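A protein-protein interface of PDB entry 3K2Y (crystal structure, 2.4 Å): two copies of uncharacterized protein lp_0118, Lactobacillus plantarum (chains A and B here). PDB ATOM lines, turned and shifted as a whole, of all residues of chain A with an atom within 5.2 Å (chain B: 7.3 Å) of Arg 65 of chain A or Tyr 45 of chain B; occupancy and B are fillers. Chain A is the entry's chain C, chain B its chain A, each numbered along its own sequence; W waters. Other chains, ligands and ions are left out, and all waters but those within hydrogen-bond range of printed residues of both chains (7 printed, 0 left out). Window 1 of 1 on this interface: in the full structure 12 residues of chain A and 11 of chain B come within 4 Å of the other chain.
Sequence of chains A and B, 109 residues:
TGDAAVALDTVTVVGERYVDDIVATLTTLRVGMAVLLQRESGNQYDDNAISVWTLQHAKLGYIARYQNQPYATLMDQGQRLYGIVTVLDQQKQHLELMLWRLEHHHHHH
Tyr 18 of chain A touches Tyr 45 of chain B, but with the chains exchanged Tyr 45 of chain A does not touch Tyr 18 of chain B (6.3 Å).
Tyr 45 of chain A touches Tyr 62 of chain B, and with the chains exchanged Tyr 62 of chain A touches Tyr 45 of chain B.
Asp 46 of chain A touches Tyr 45 of chain B, but with the chains exchanged Tyr 45 of chain A does not touch Asp 46 of chain B (7.7 Å).
Arg 65 of chain A touches Tyr 18 of chain B, but with the chains exchanged Tyr 18 of chain A does not touch Arg 65 of chain B (5.7 Å).
Of the 20 pairs that touch across the chains among the printed residues, 2 have their exchanged pair printed and touching as well.
Tyr 18 of chain A touches Gln 44 of chain B.
CE2 of Tyr 18 of chain A touches O of Tyr 45 of chain B, 3.3 Å away.
Tyr 18 of chain A touches Asp 47 of chain B.
CD1 of Tyr 45 of chain A touches OE1 of Glu 40 of chain B, at 3.2 Å.
CB of Tyr 45 of chain A touches ND2 of Asn 43 of chain B, 3.8 Å away.
CD2 of Tyr 45 of chain A touches OE1 of Gln 44 of chain B, 3.2 Å away.
Tyr 45 of chain A touches Tyr 62 of chain B (CB to OH, 3.7 Å).
CB of Ala 49 of chain A touches NE2 of Gln 44 of chain B, at 3.7 Å.
Tyr 18 of chain B touches Arg 65 of chain A (CE1 to O, 3.7 Å).
OH of Tyr 18 of chain B touches CA of Tyr 66 of chain A, at 3.2 Å.
NZ of Lys 59 of chain B lies within hydrogen-bond range of O of Tyr 45 of chain A (3.5 Å).
The side-chain amide oxygen (OD1) of Asn 68 of chain A lies within hydrogen-bond range of the side-chain hydroxyl (OH) of Tyr 45 of chain B.
OH of Tyr 45 of chain B sits at hydrogen-bond distance from OD2 of Asp 46 of chain A.
OD1 of Asp 46 of chain B sits at hydrogen-bond distance from N of Asn 48 of chain B.
The side-chain amide nitrogen (ND2) of Asn 68 of chain A is in hydrogen-bond range of the backbone carbonyl oxygen (O) of Ile 63 of chain A.
O of Tyr 45 of chain A lies within hydrogen-bond range of NH2 of Arg 65 of chain A (2.5 Å).
The backbone NH of Tyr 45 of chain B lies within hydrogen-bond range of the side-chain amide oxygen of Asn 43 of chain B (2.7 Å).
N of Val 14 of chain A lies within hydrogen-bond range of O of Tyr 62 of chain A, at 2.5 Å.
O of Ala 64 of chain A is in hydrogen-bond range of ND2 of Asn 68 of chain A.
Hydrophobic or aromatic side chains of chain B within 4 Å of the printed part of chain A: Tyr 18, Tyr 45 and Tyr 62.
Along chain B the printed residues that touch a printed residue of chain A span positions 18 to 62.
Of the 15 printed residues of chain A, 10 touch a printed residue of chain B.
Hydrophobic or aromatic side chains of chain A within 4 Å of the printed part of chain B: Val 14, Tyr 18, Tyr 45, Ala 49, Tyr 62 and Tyr 66.
Water W7 lies within hydrogen-bond range of N of Gly 42 of chain B (2.6 Å) and OH of Tyr 45 of chain A (3.0 Å).
Water W1 lies within hydrogen-bond range of the backbone carbonyl oxygen of Tyr 45 of chain B, the side-chain hydroxyl of Tyr 18 of chain A and the guanidinium group of Arg 65 of chain B.
Water W6 lies within hydrogen-bond range of O of Gln 44 of chain B (2.8 Å) and O of Gly 15 of chain A (3.1 Å).
Water W5 lies within hydrogen-bond range of the side-chain amide nitrogen of Asn 68 of chain A (2.8 Å), the backbone NH of Ile 50 of chain A (2.8 Å), the side-chain hydroxyl of Tyr 45 of chain B (2.9 Å) and the backbone carbonyl oxygen of Ile 63 of chain A (3.0 Å).
Water W4 lies within hydrogen-bond range of the side-chain amino group of Lys 59 of chain B (2.9 Å) and the backbone carbonyl oxygen of Tyr 45 of chain A (3.4 Å).
Water W3 lies within hydrogen-bond range of NZ of Lys 59 of chain B and NH2 of Arg 65 of chain A.
Arg 65 of chain A touches just these residues of chain B: Tyr 18 and Tyr 45.
Of chain A, only Val 14 (3.8 Å), Tyr 18 (3.3 Å), Asp 46 (2.7 Å), Tyr 62 (3.9 Å), Arg 65 (3.4 Å) and Asn 68 (3.5 Å) come within 4 Å of Tyr 45 of chain B.
Of the printed residues of chain A, Tyr 18 of chain B touches Arg 65 (3.7 Å) and Tyr 66 (3.2 Å).
Printed residues of chain A within 4 Å of Tyr 62 of chain B: Tyr 45 (3.7 Å).
Of the printed residues of chain A, Glu 40 of chain B touches Tyr 45.
Of the printed residues of chain A, Gly 42 of chain B touches Tyr 45 (3.4 Å).
Printed residues of chain B within 4 Å of Gly 15 of chain A: Gln 44 (3.4 Å).
Ala 64 of chain A touches none of the printed residues of chain B.
Ala 49 of chain B touches none of the printed residues of chain A.
The nearest residue of chain B that does not touch Arg 65 of chain A is Tyr 62 of chain B (4.2 Å).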
ATOM      1  N   VAL A  14       8.912 -34.254   1.712  1.00  0.00           N
ATOM      2  CA  VAL A  14      10.076 -33.870   0.926  1.00  0.00           C
ATOM      3  C   VAL A  14      11.370 -33.955   1.737  1.00  0.00           C
ATOM      4  O   VAL A  14      11.353 -34.281   2.925  1.00  0.00           O
ATOM      5  CB  VAL A  14       9.924 -32.417   0.394  1.00  0.00           C
ATOM      6  CG1 VAL A  14       8.720 -32.316  -0.544  1.00  0.00           C
ATOM      7  CG2 VAL A  14       9.759 -31.448   1.565  1.00  0.00           C
ATOM      8  N   GLY A  15      12.490 -33.666   1.073  1.00  0.00           N
ATOM      9  CA  GLY A  15      13.789 -33.686   1.723  1.00  0.00           C
ATOM     10  C   GLY A  15      14.376 -35.051   2.034  1.00  0.00           C
ATOM     11  O   GLY A  15      15.420 -35.137   2.680  1.00  0.00           O
ATOM     12  N   TYR A  18      18.104 -35.683   1.780  1.00  0.00           N
ATOM     13  CA  TYR A  18      18.983 -35.022   2.736  1.00  0.00           C
ATOM     14  C   TYR A  18      18.909 -35.654   4.116  1.00  0.00           C
ATOM     15  O   TYR A  18      19.427 -35.104   5.088  1.00  0.00           O
ATOM     16  CB  TYR A  18      18.623 -33.539   2.819  1.00  0.00           C
ATOM     17  CG  TYR A  18      18.433 -32.906   1.463  1.00  0.00           C
ATOM     18  CD1 TYR A  18      19.491 -32.820   0.556  1.00  0.00           C
ATOM     19  CD2 TYR A  18      17.182 -32.432   1.065  1.00  0.00           C
ATOM     20  CE1 TYR A  18      19.304 -32.280  -0.720  1.00  0.00           C
ATOM     21  CE2 TYR A  18      16.985 -31.892  -0.209  1.00  0.00           C
ATOM     22  CZ  TYR A  18      18.049 -31.821  -1.091  1.00  0.00           C
ATOM     23  OH  TYR A  18      17.857 -31.297  -2.348  1.00  0.00           O
ATOM     24  N   TYR A  45      14.820 -22.428   9.628  1.00  0.00           N
ATOM     25  CA  TYR A  45      14.538 -22.120   8.234  1.00  0.00           C
ATOM     26  C   TYR A  45      13.049 -21.934   7.962  1.00  0.00           C
ATOM     27  O   TYR A  45      12.659 -21.214   7.042  1.00  0.00           O
ATOM     28  CB  TYR A  45      15.101 -23.241   7.356  1.00  0.00           C
ATOM     29  CG  TYR A  45      16.476 -23.704   7.793  1.00  0.00           C
ATOM     30  CD1 TYR A  45      17.596 -22.885   7.641  1.00  0.00           C
ATOM     31  CD2 TYR A  45      16.652 -24.950   8.385  1.00  0.00           C
ATOM     32  CE1 TYR A  45      18.858 -23.300   8.072  1.00  0.00           C
ATOM     33  CE2 TYR A  45      17.904 -25.377   8.821  1.00  0.00           C
ATOM     34  CZ  TYR A  45      19.002 -24.549   8.663  1.00  0.00           C
ATOM     35  OH  TYR A  45      20.236 -24.970   9.107  1.00  0.00           O
ATOM     36  N   ASP A  46      12.218 -22.568   8.781  1.00  0.00           N
ATOM     37  CA  ASP A  46      10.775 -22.500   8.598  1.00  0.00           C
ATOM     38  C   ASP A  46      10.068 -22.858   9.902  1.00  0.00           C
ATOM     39  O   ASP A  46      10.100 -24.010  10.332  1.00  0.00           O
ATOM     40  CB  ASP A  46      10.398 -23.466   7.467  1.00  0.00           C
ATOM     41  CG  ASP A  46       8.915 -23.707   7.359  1.00  0.00           C
ATOM     42  OD1 ASP A  46       8.128 -22.792   7.676  1.00  0.00           O
ATOM     43  OD2 ASP A  46       8.540 -24.820   6.931  1.00  0.00           O
ATOM     44  N   ALA A  49       7.715 -25.818  10.244  1.00  0.00           N
ATOM     45  CA  ALA A  49       8.360 -27.103   9.995  1.00  0.00           C
ATOM     46  C   ALA A  49       7.720 -28.270  10.730  1.00  0.00           C
ATOM     47  O   ALA A  49       7.419 -28.178  11.921  1.00  0.00           O
ATOM     48  CB  ALA A  49       9.826 -27.021  10.355  1.00  0.00           C
ATOM     49  N   ILE A  50       7.527 -29.366   9.999  1.00  0.00           N
ATOM     50  CA  ILE A  50       6.948 -30.595  10.530  1.00  0.00           C
ATOM     51  C   ILE A  50       7.680 -31.777   9.897  1.00  0.00           C
ATOM     52  O   ILE A  50       7.542 -32.041   8.702  1.00  0.00           O
ATOM     53  CB  ILE A  50       5.442 -30.718  10.196  1.00  0.00           C
ATOM     54  CG1 ILE A  50       4.682 -29.493  10.706  1.00  0.00           C
ATOM     55  CG2 ILE A  50       4.868 -31.969  10.849  1.00  0.00           C
ATOM     56  CD1 ILE A  50       3.207 -29.498  10.339  1.00  0.00           C
ATOM     57  N   TYR A  62      10.362 -34.176   5.581  1.00  0.00           N
ATOM     58  CA  TYR A  62       9.447 -33.138   6.041  1.00  0.00           C
ATOM     59  C   TYR A  62       8.236 -32.943   5.144  1.00  0.00           C
ATOM     60  O   TYR A  62       8.256 -33.296   3.970  1.00  0.00           O
ATOM     61  CB  TYR A  62      10.174 -31.792   6.158  1.00  0.00           C
ATOM     62  CG  TYR A  62      11.152 -31.702   7.303  1.00  0.00           C
ATOM     63  CD1 TYR A  62      12.356 -32.399   7.277  1.00  0.00           C
ATOM     64  CD2 TYR A  62      10.861 -30.925   8.423  1.00  0.00           C
ATOM     65  CE1 TYR A  62      13.253 -32.327   8.342  1.00  0.00           C
ATOM     66  CE2 TYR A  62      11.746 -30.845   9.496  1.00  0.00           C
ATOM     67  CZ  TYR A  62      12.939 -31.546   9.451  1.00  0.00           C
ATOM     68  OH  TYR A  62      13.812 -31.470  10.517  1.00  0.00           O
ATOM     69  N   ILE A  63       7.177 -32.376   5.714  1.00  0.00           N
ATOM     70  CA  ILE A  63       5.968 -32.091   4.957  1.00  0.00           C
ATOM     71  C   ILE A  63       6.300 -30.863   4.111  1.00  0.00           C
ATOM     72  O   ILE A  63       6.868 -29.894   4.617  1.00  0.00           O
ATOM     73  CB  ILE A  63       4.780 -31.788   5.899  1.00  0.00           C
ATOM     74  CG1 ILE A  63       4.338 -33.080   6.602  1.00  0.00           C
ATOM     75  CG2 ILE A  63       3.625 -31.176   5.118  1.00  0.00           C
ATOM     76  CD1 ILE A  63       3.257 -32.880   7.643  1.00  0.00           C
ATOM     77  N   ALA A  64       5.968 -30.917   2.824  1.00  0.00           N
ATOM     78  CA  ALA A  64       6.249 -29.816   1.911  1.00  0.00           C
ATOM     79  C   ALA A  64       5.965 -28.457   2.538  1.00  0.00           C
ATOM     80  O   ALA A  64       5.049 -28.308   3.350  1.00  0.00           O
ATOM     81  CB  ALA A  64       5.443 -29.979   0.633  1.00  0.00           C
ATOM     82  N   ARG A  65       6.756 -27.465   2.153  1.00  0.00           N
ATOM     83  CA  ARG A  65       6.595 -26.121   2.684  1.00  0.00           C
ATOM     84  C   ARG A  65       5.255 -25.516   2.268  1.00  0.00           C
ATOM     85  O   ARG A  65       4.652 -24.756   3.028  1.00  0.00           O
ATOM     86  CB  ARG A  65       7.747 -25.234   2.201  1.00  0.00           C
ATOM     87  CG  ARG A  65       7.890 -23.917   2.938  1.00  0.00           C
ATOM     88  CD  ARG A  65       9.170 -23.232   2.527  1.00  0.00           C
ATOM     89  NE  ARG A  65       9.800 -22.533   3.644  1.00  0.00           N
ATOM     90  CZ  ARG A  65      11.114 -22.424   3.793  1.00  0.00           C
ATOM     91  NH1 ARG A  65      11.927 -22.969   2.896  1.00  0.00           N
ATOM     92  NH2 ARG A  65      11.618 -21.782   4.833  1.00  0.00           N
ATOM     93  N   TYR A  66       4.787 -25.861   1.070  1.00  0.00           N
ATOM     94  CA  TYR A  66       3.518 -25.335   0.574  1.00  0.00           C
ATOM     95  C   TYR A  66       2.301 -26.037   1.165  1.00  0.00           C
ATOM     96  O   TYR A  66       1.167 -25.716   0.816  1.00  0.00           O
ATOM     97  CB  TYR A  66       3.460 -25.407  -0.961  1.00  0.00           C
ATOM     98  CG  TYR A  66       3.913 -26.722  -1.561  1.00  0.00           C
ATOM     99  CD1 TYR A  66       5.271 -27.017  -1.699  1.00  0.00           C
ATOM    100  CD2 TYR A  66       2.984 -27.667  -2.004  1.00  0.00           C
ATOM    101  CE1 TYR A  66       5.695 -28.219  -2.269  1.00  0.00           C
ATOM    102  CE2 TYR A  66       3.394 -28.874  -2.571  1.00  0.00           C
ATOM    103  CZ  TYR A  66       4.750 -29.144  -2.702  1.00  0.00           C
ATOM    104  OH  TYR A  66       5.168 -30.333  -3.269  1.00  0.00           O
ATOM    105  N   GLN A  67       2.544 -26.989   2.064  1.00  0.00           N
ATOM    106  CA  GLN A  67       1.477 -27.741   2.720  1.00  0.00           C
ATOM    107  C   GLN A  67       1.674 -27.741   4.236  1.00  0.00           C
ATOM    108  O   GLN A  67       1.028 -28.487   4.962  1.00  0.00           O
ATOM    109  CB  GLN A  67       1.462 -29.175   2.187  1.00  0.00           C
ATOM    110  CG  GLN A  67       1.014 -29.273   0.736  1.00  0.00           C
ATOM    111  CD  GLN A  67       1.303 -30.624   0.104  1.00  0.00           C
ATOM    112  OE1 GLN A  67       0.723 -30.970  -0.924  1.00  0.00           O
ATOM    113  NE2 GLN A  67       2.215 -31.384   0.704  1.00  0.00           N
ATOM    114  N   ASN A  68       2.576 -26.881   4.693  1.00  0.00           N
ATOM    115  CA  ASN A  68       2.926 -26.719   6.104  1.00  0.00           C
ATOM    116  C   ASN A  68       1.854 -26.100   7.000  1.00  0.00           C
ATOM    117  O   ASN A  68       1.271 -26.768   7.858  1.00  0.00           O
ATOM    118  CB  ASN A  68       4.181 -25.844   6.209  1.00  0.00           C
ATOM    119  CG  ASN A  68       5.424 -26.643   6.470  1.00  0.00           C
ATOM    120  OD1 ASN A  68       6.536 -26.118   6.428  1.00  0.00           O
ATOM    121  ND2 ASN A  68       5.246 -27.925   6.755  1.00  0.00           N
ATOM    122  N   GLN A  69       1.645 -24.800   6.792  1.00  0.00           N
ATOM    123  CA  GLN A  69       0.714 -23.964   7.553  1.00  0.00           C
ATOM    124  C   GLN A  69      -0.561 -24.604   8.106  1.00  0.00           C
ATOM    125  O   GLN A  69      -0.739 -24.667   9.321  1.00  0.00           O
ATOM    126  CB  GLN A  69       0.360 -22.718   6.723  1.00  0.00           C
ATOM    127  CG  GLN A  69      -0.400 -21.626   7.472  1.00  0.00           C
ATOM    128  CD  GLN A  69      -1.888 -21.916   7.604  1.00  0.00           C
ATOM    129  OE1 GLN A  69      -2.590 -22.091   6.605  1.00  0.00           O
ATOM    130  NE2 GLN A  69      -2.376 -21.962   8.840  1.00  0.00           N
ATOM    131  N   GLY B  15      10.620 -17.534  -2.556  1.00  0.00           N
ATOM    132  CA  GLY B  15      10.196 -17.849  -1.204  1.00  0.00           C
ATOM    133  C   GLY B  15       9.735 -16.689  -0.340  1.00  0.00           C
ATOM    134  O   GLY B  15       9.520 -16.870   0.859  1.00  0.00           O
ATOM    135  N   TYR B  18       6.783 -16.940   2.100  1.00  0.00           N
ATOM    136  CA  TYR B  18       7.007 -17.669   3.343  1.00  0.00           C
ATOM    137  C   TYR B  18       7.744 -16.851   4.397  1.00  0.00           C
ATOM    138  O   TYR B  18       7.977 -17.326   5.510  1.00  0.00           O
ATOM    139  CB  TYR B  18       7.772 -18.962   3.052  1.00  0.00           C
ATOM    140  CG  TYR B  18       7.002 -19.920   2.169  1.00  0.00           C
ATOM    141  CD1 TYR B  18       5.779 -20.452   2.588  1.00  0.00           C
ATOM    142  CD2 TYR B  18       7.479 -20.280   0.909  1.00  0.00           C
ATOM    143  CE1 TYR B  18       5.049 -21.313   1.776  1.00  0.00           C
ATOM    144  CE2 TYR B  18       6.757 -21.145   0.088  1.00  0.00           C
ATOM    145  CZ  TYR B  18       5.540 -21.656   0.526  1.00  0.00           C
ATOM    146  OH  TYR B  18       4.810 -22.500  -0.285  1.00  0.00           O
ATOM    147  N   VAL B  19       8.103 -15.620   4.043  1.00  0.00           N
ATOM    148  CA  VAL B  19       8.810 -14.729   4.960  1.00  0.00           C
ATOM    149  C   VAL B  19       7.821 -13.838   5.709  1.00  0.00           C
ATOM    150  O   VAL B  19       7.079 -13.069   5.100  1.00  0.00           O
ATOM    151  CB  VAL B  19       9.816 -13.837   4.209  1.00  0.00           C
ATOM    152  CG1 VAL B  19      10.549 -12.941   5.196  1.00  0.00           C
ATOM    153  CG2 VAL B  19      10.803 -14.706   3.431  1.00  0.00           C
ATOM    154  N   GLU B  40      23.003 -22.347   3.948  1.00  0.00           N
ATOM    155  CA  GLU B  40      22.278 -23.196   4.885  1.00  0.00           C
ATOM    156  C   GLU B  40      22.325 -24.639   4.388  1.00  0.00           C
ATOM    157  O   GLU B  40      21.346 -25.158   3.855  1.00  0.00           O
ATOM    158  CB  GLU B  40      20.827 -22.720   5.017  1.00  0.00           C
ATOM    159  CG  GLU B  40      20.690 -21.225   5.240  1.00  0.00           C
ATOM    160  CD  GLU B  40      19.251 -20.787   5.477  1.00  0.00           C
ATOM    161  OE1 GLU B  40      18.335 -21.382   4.871  1.00  0.00           O
ATOM    162  OE2 GLU B  40      19.040 -19.834   6.257  1.00  0.00           O
ATOM    163  N   GLY B  42      22.204 -27.052   6.031  1.00  0.00           N
ATOM    164  CA  GLY B  42      21.367 -27.845   6.913  1.00  0.00           C
ATOM    165  C   GLY B  42      19.883 -27.681   6.607  1.00  0.00           C
ATOM    166  O   GLY B  42      19.033 -28.247   7.298  1.00  0.00           O
ATOM    167  N   ASN B  43      19.565 -26.906   5.572  1.00  0.00           N
ATOM    168  CA  ASN B  43      18.171 -26.691   5.192  1.00  0.00           C
ATOM    169  C   ASN B  43      17.554 -28.046   4.817  1.00  0.00           C
ATOM    170  O   ASN B  43      18.048 -28.742   3.928  1.00  0.00           O
ATOM    171  CB  ASN B  43      18.090 -25.703   4.019  1.00  0.00           C
ATOM    172  CG  ASN B  43      16.660 -25.286   3.700  1.00  0.00           C
ATOM    173  OD1 ASN B  43      15.834 -26.115   3.316  1.00  0.00           O
ATOM    174  ND2 ASN B  43      16.365 -23.997   3.857  1.00  0.00           N
ATOM    175  N   GLN B  44      16.479 -28.416   5.509  1.00  0.00           N
ATOM    176  CA  GLN B  44      15.822 -29.695   5.271  1.00  0.00           C
ATOM    177  C   GLN B  44      15.190 -29.830   3.890  1.00  0.00           C
ATOM    178  O   GLN B  44      14.889 -30.939   3.450  1.00  0.00           O
ATOM    179  CB  GLN B  44      14.755 -29.963   6.344  1.00  0.00           C
ATOM    180  CG  GLN B  44      13.587 -28.986   6.344  1.00  0.00           C
ATOM    181  CD  GLN B  44      13.702 -27.925   7.425  1.00  0.00           C
ATOM    182  OE1 GLN B  44      14.800 -27.468   7.754  1.00  0.00           O
ATOM    183  NE2 GLN B  44      12.564 -27.516   7.974  1.00  0.00           N
ATOM    184  N   TYR B  45      14.999 -28.715   3.196  1.00  0.00           N
ATOM    185  CA  TYR B  45      14.379 -28.768   1.878  1.00  0.00           C
ATOM    186  C   TYR B  45      15.401 -28.755   0.744  1.00  0.00           C
ATOM    187  O   TYR B  45      15.117 -29.217  -0.362  1.00  0.00           O
ATOM    188  CB  TYR B  45      13.405 -27.591   1.712  1.00  0.00           C
ATOM    189  CG  TYR B  45      12.432 -27.441   2.864  1.00  0.00           C
ATOM    190  CD1 TYR B  45      11.561 -28.477   3.206  1.00  0.00           C
ATOM    191  CD2 TYR B  45      12.409 -26.278   3.636  1.00  0.00           C
ATOM    192  CE1 TYR B  45      10.688 -28.365   4.295  1.00  0.00           C
ATOM    193  CE2 TYR B  45      11.541 -26.151   4.727  1.00  0.00           C
ATOM    194  CZ  TYR B  45      10.685 -27.205   5.051  1.00  0.00           C
ATOM    195  OH  TYR B  45       9.842 -27.100   6.135  1.00  0.00           O
ATOM    196  N   ASP B  46      16.592 -28.236   1.025  1.00  0.00           N
ATOM    197  CA  ASP B  46      17.639 -28.148   0.011  1.00  0.00           C
ATOM    198  C   ASP B  46      19.001 -27.975   0.674  1.00  0.00           C
ATOM    199  O   ASP B  46      19.261 -26.955   1.310  1.00  0.00           O
ATOM    200  CB  ASP B  46      17.367 -26.952  -0.906  1.00  0.00           C
ATOM    201  CG  ASP B  46      18.260 -26.933  -2.132  1.00  0.00           C
ATOM    202  OD1 ASP B  46      19.320 -27.593  -2.116  1.00  0.00           O
ATOM    203  OD2 ASP B  46      17.904 -26.245  -3.112  1.00  0.00           O
ATOM    204  N   ASP B  47      19.876 -28.962   0.515  1.00  0.00           N
ATOM    205  CA  ASP B  47      21.202 -28.884   1.117  1.00  0.00           C
ATOM    206  C   ASP B  47      22.077 -27.838   0.428  1.00  0.00           C
ATOM    207  O   ASP B  47      23.171 -27.541   0.891  1.00  0.00           O
ATOM    208  CB  ASP B  47      21.887 -30.257   1.080  1.00  0.00           C
ATOM    209  CG  ASP B  47      22.250 -30.697  -0.325  1.00  0.00           C
ATOM    210  OD1 ASP B  47      21.678 -30.162  -1.297  1.00  0.00           O
ATOM    211  OD2 ASP B  47      23.105 -31.596  -0.457  1.00  0.00           O
ATOM    212  N   ASN B  48      21.586 -27.278  -0.671  1.00  0.00           N
ATOM    213  CA  ASN B  48      22.330 -26.258  -1.409  1.00  0.00           C
ATOM    214  C   ASN B  48      21.762 -24.874  -1.159  1.00  0.00           C
ATOM    215  O   ASN B  48      22.224 -23.884  -1.733  1.00  0.00           O
ATOM    216  CB  ASN B  48      22.294 -26.554  -2.907  1.00  0.00           C
ATOM    217  CG  ASN B  48      23.292 -27.616  -3.313  1.00  0.00           C
ATOM    218  OD1 ASN B  48      22.939 -28.581  -3.981  1.00  0.00           O
ATOM    219  ND2 ASN B  48      24.548 -27.440  -2.918  1.00  0.00           N
ATOM    220  N   ALA B  49      20.758 -24.825  -0.288  1.00  0.00           N
ATOM    221  CA  ALA B  49      20.071 -23.595   0.076  1.00  0.00           C
ATOM    222  C   ALA B  49      20.992 -22.440   0.440  1.00  0.00           C
ATOM    223  O   ALA B  49      22.062 -22.628   1.029  1.00  0.00           O
ATOM    224  CB  ALA B  49      19.115 -23.862   1.234  1.00  0.00           C
ATOM    225  N   LYS B  59      15.328 -11.366   6.767  1.00  0.00           N
ATOM    226  CA  LYS B  59      15.240 -12.346   5.694  1.00  0.00           C
ATOM    227  C   LYS B  59      14.389 -11.872   4.524  1.00  0.00           C
ATOM    228  O   LYS B  59      13.343 -11.253   4.711  1.00  0.00           O
ATOM    229  CB  LYS B  59      14.696 -13.665   6.235  1.00  0.00           C
ATOM    230  CG  LYS B  59      14.885 -14.836   5.292  1.00  0.00           C
ATOM    231  CD  LYS B  59      14.495 -16.137   5.956  1.00  0.00           C
ATOM    232  CE  LYS B  59      14.951 -17.329   5.130  1.00  0.00           C
ATOM    233  NZ  LYS B  59      14.644 -18.618   5.806  1.00  0.00           N
ATOM    234  N   TYR B  62      15.230 -16.907  -0.603  1.00  0.00           N
ATOM    235  CA  TYR B  62      16.307 -17.811  -0.994  1.00  0.00           C
ATOM    236  C   TYR B  62      16.698 -17.634  -2.446  1.00  0.00           C
ATOM    237  O   TYR B  62      15.937 -17.079  -3.239  1.00  0.00           O
ATOM    238  CB  TYR B  62      15.884 -19.270  -0.807  1.00  0.00           C
ATOM    239  CG  TYR B  62      15.802 -19.712   0.626  1.00  0.00           C
ATOM    240  CD1 TYR B  62      14.681 -19.432   1.404  1.00  0.00           C
ATOM    241  CD2 TYR B  62      16.868 -20.382   1.220  1.00  0.00           C
ATOM    242  CE1 TYR B  62      14.627 -19.806   2.742  1.00  0.00           C
ATOM    243  CE2 TYR B  62      16.825 -20.757   2.553  1.00  0.00           C
ATOM    244  CZ  TYR B  62      15.706 -20.465   3.310  1.00  0.00           C
ATOM    245  OH  TYR B  62      15.690 -20.806   4.639  1.00  0.00           O
ATOM    246  N   ARG B  65      16.212 -22.367  -6.572  1.00  0.00           N
ATOM    247  CA  ARG B  65      16.788 -23.713  -6.615  1.00  0.00           C
ATOM    248  C   ARG B  65      17.527 -24.060  -7.908  1.00  0.00           C
ATOM    249  O   ARG B  65      18.476 -24.848  -7.891  1.00  0.00           O
ATOM    250  CB  ARG B  65      15.695 -24.755  -6.350  1.00  0.00           C
ATOM    251  CG  ARG B  65      16.171 -26.199  -6.401  1.00  0.00           C
ATOM    252  CD  ARG B  65      15.064 -27.162  -6.000  1.00  0.00           C
ATOM    253  NE  ARG B  65      14.722 -27.045  -4.584  1.00  0.00           N
ATOM    254  CZ  ARG B  65      13.695 -27.663  -4.005  1.00  0.00           C
ATOM    255  NH1 ARG B  65      12.896 -28.446  -4.720  1.00  0.00           N
ATOM    256  NH2 ARG B  65      13.465 -27.498  -2.711  1.00  0.00           N
HETATM  257  O   HOH W   1      15.605 -29.586  -3.016  1.00  0.00           O
HETATM  258  O   HOH W   2      14.098 -23.523   1.605  1.00  0.00           O
HETATM  259  O   HOH W   3      11.772 -18.467   4.906  1.00  0.00           O
HETATM  260  O   HOH W   4      13.750 -18.351   8.573  1.00  0.00           O
HETATM  261  O   HOH W   5       7.826 -28.886   7.241  1.00  0.00           O
HETATM  262  O   HOH W   6      15.313 -33.181   5.063  1.00  0.00           O
HETATM  263  O   HOH W   7      22.815 -25.081   7.647  1.00  0.00           O
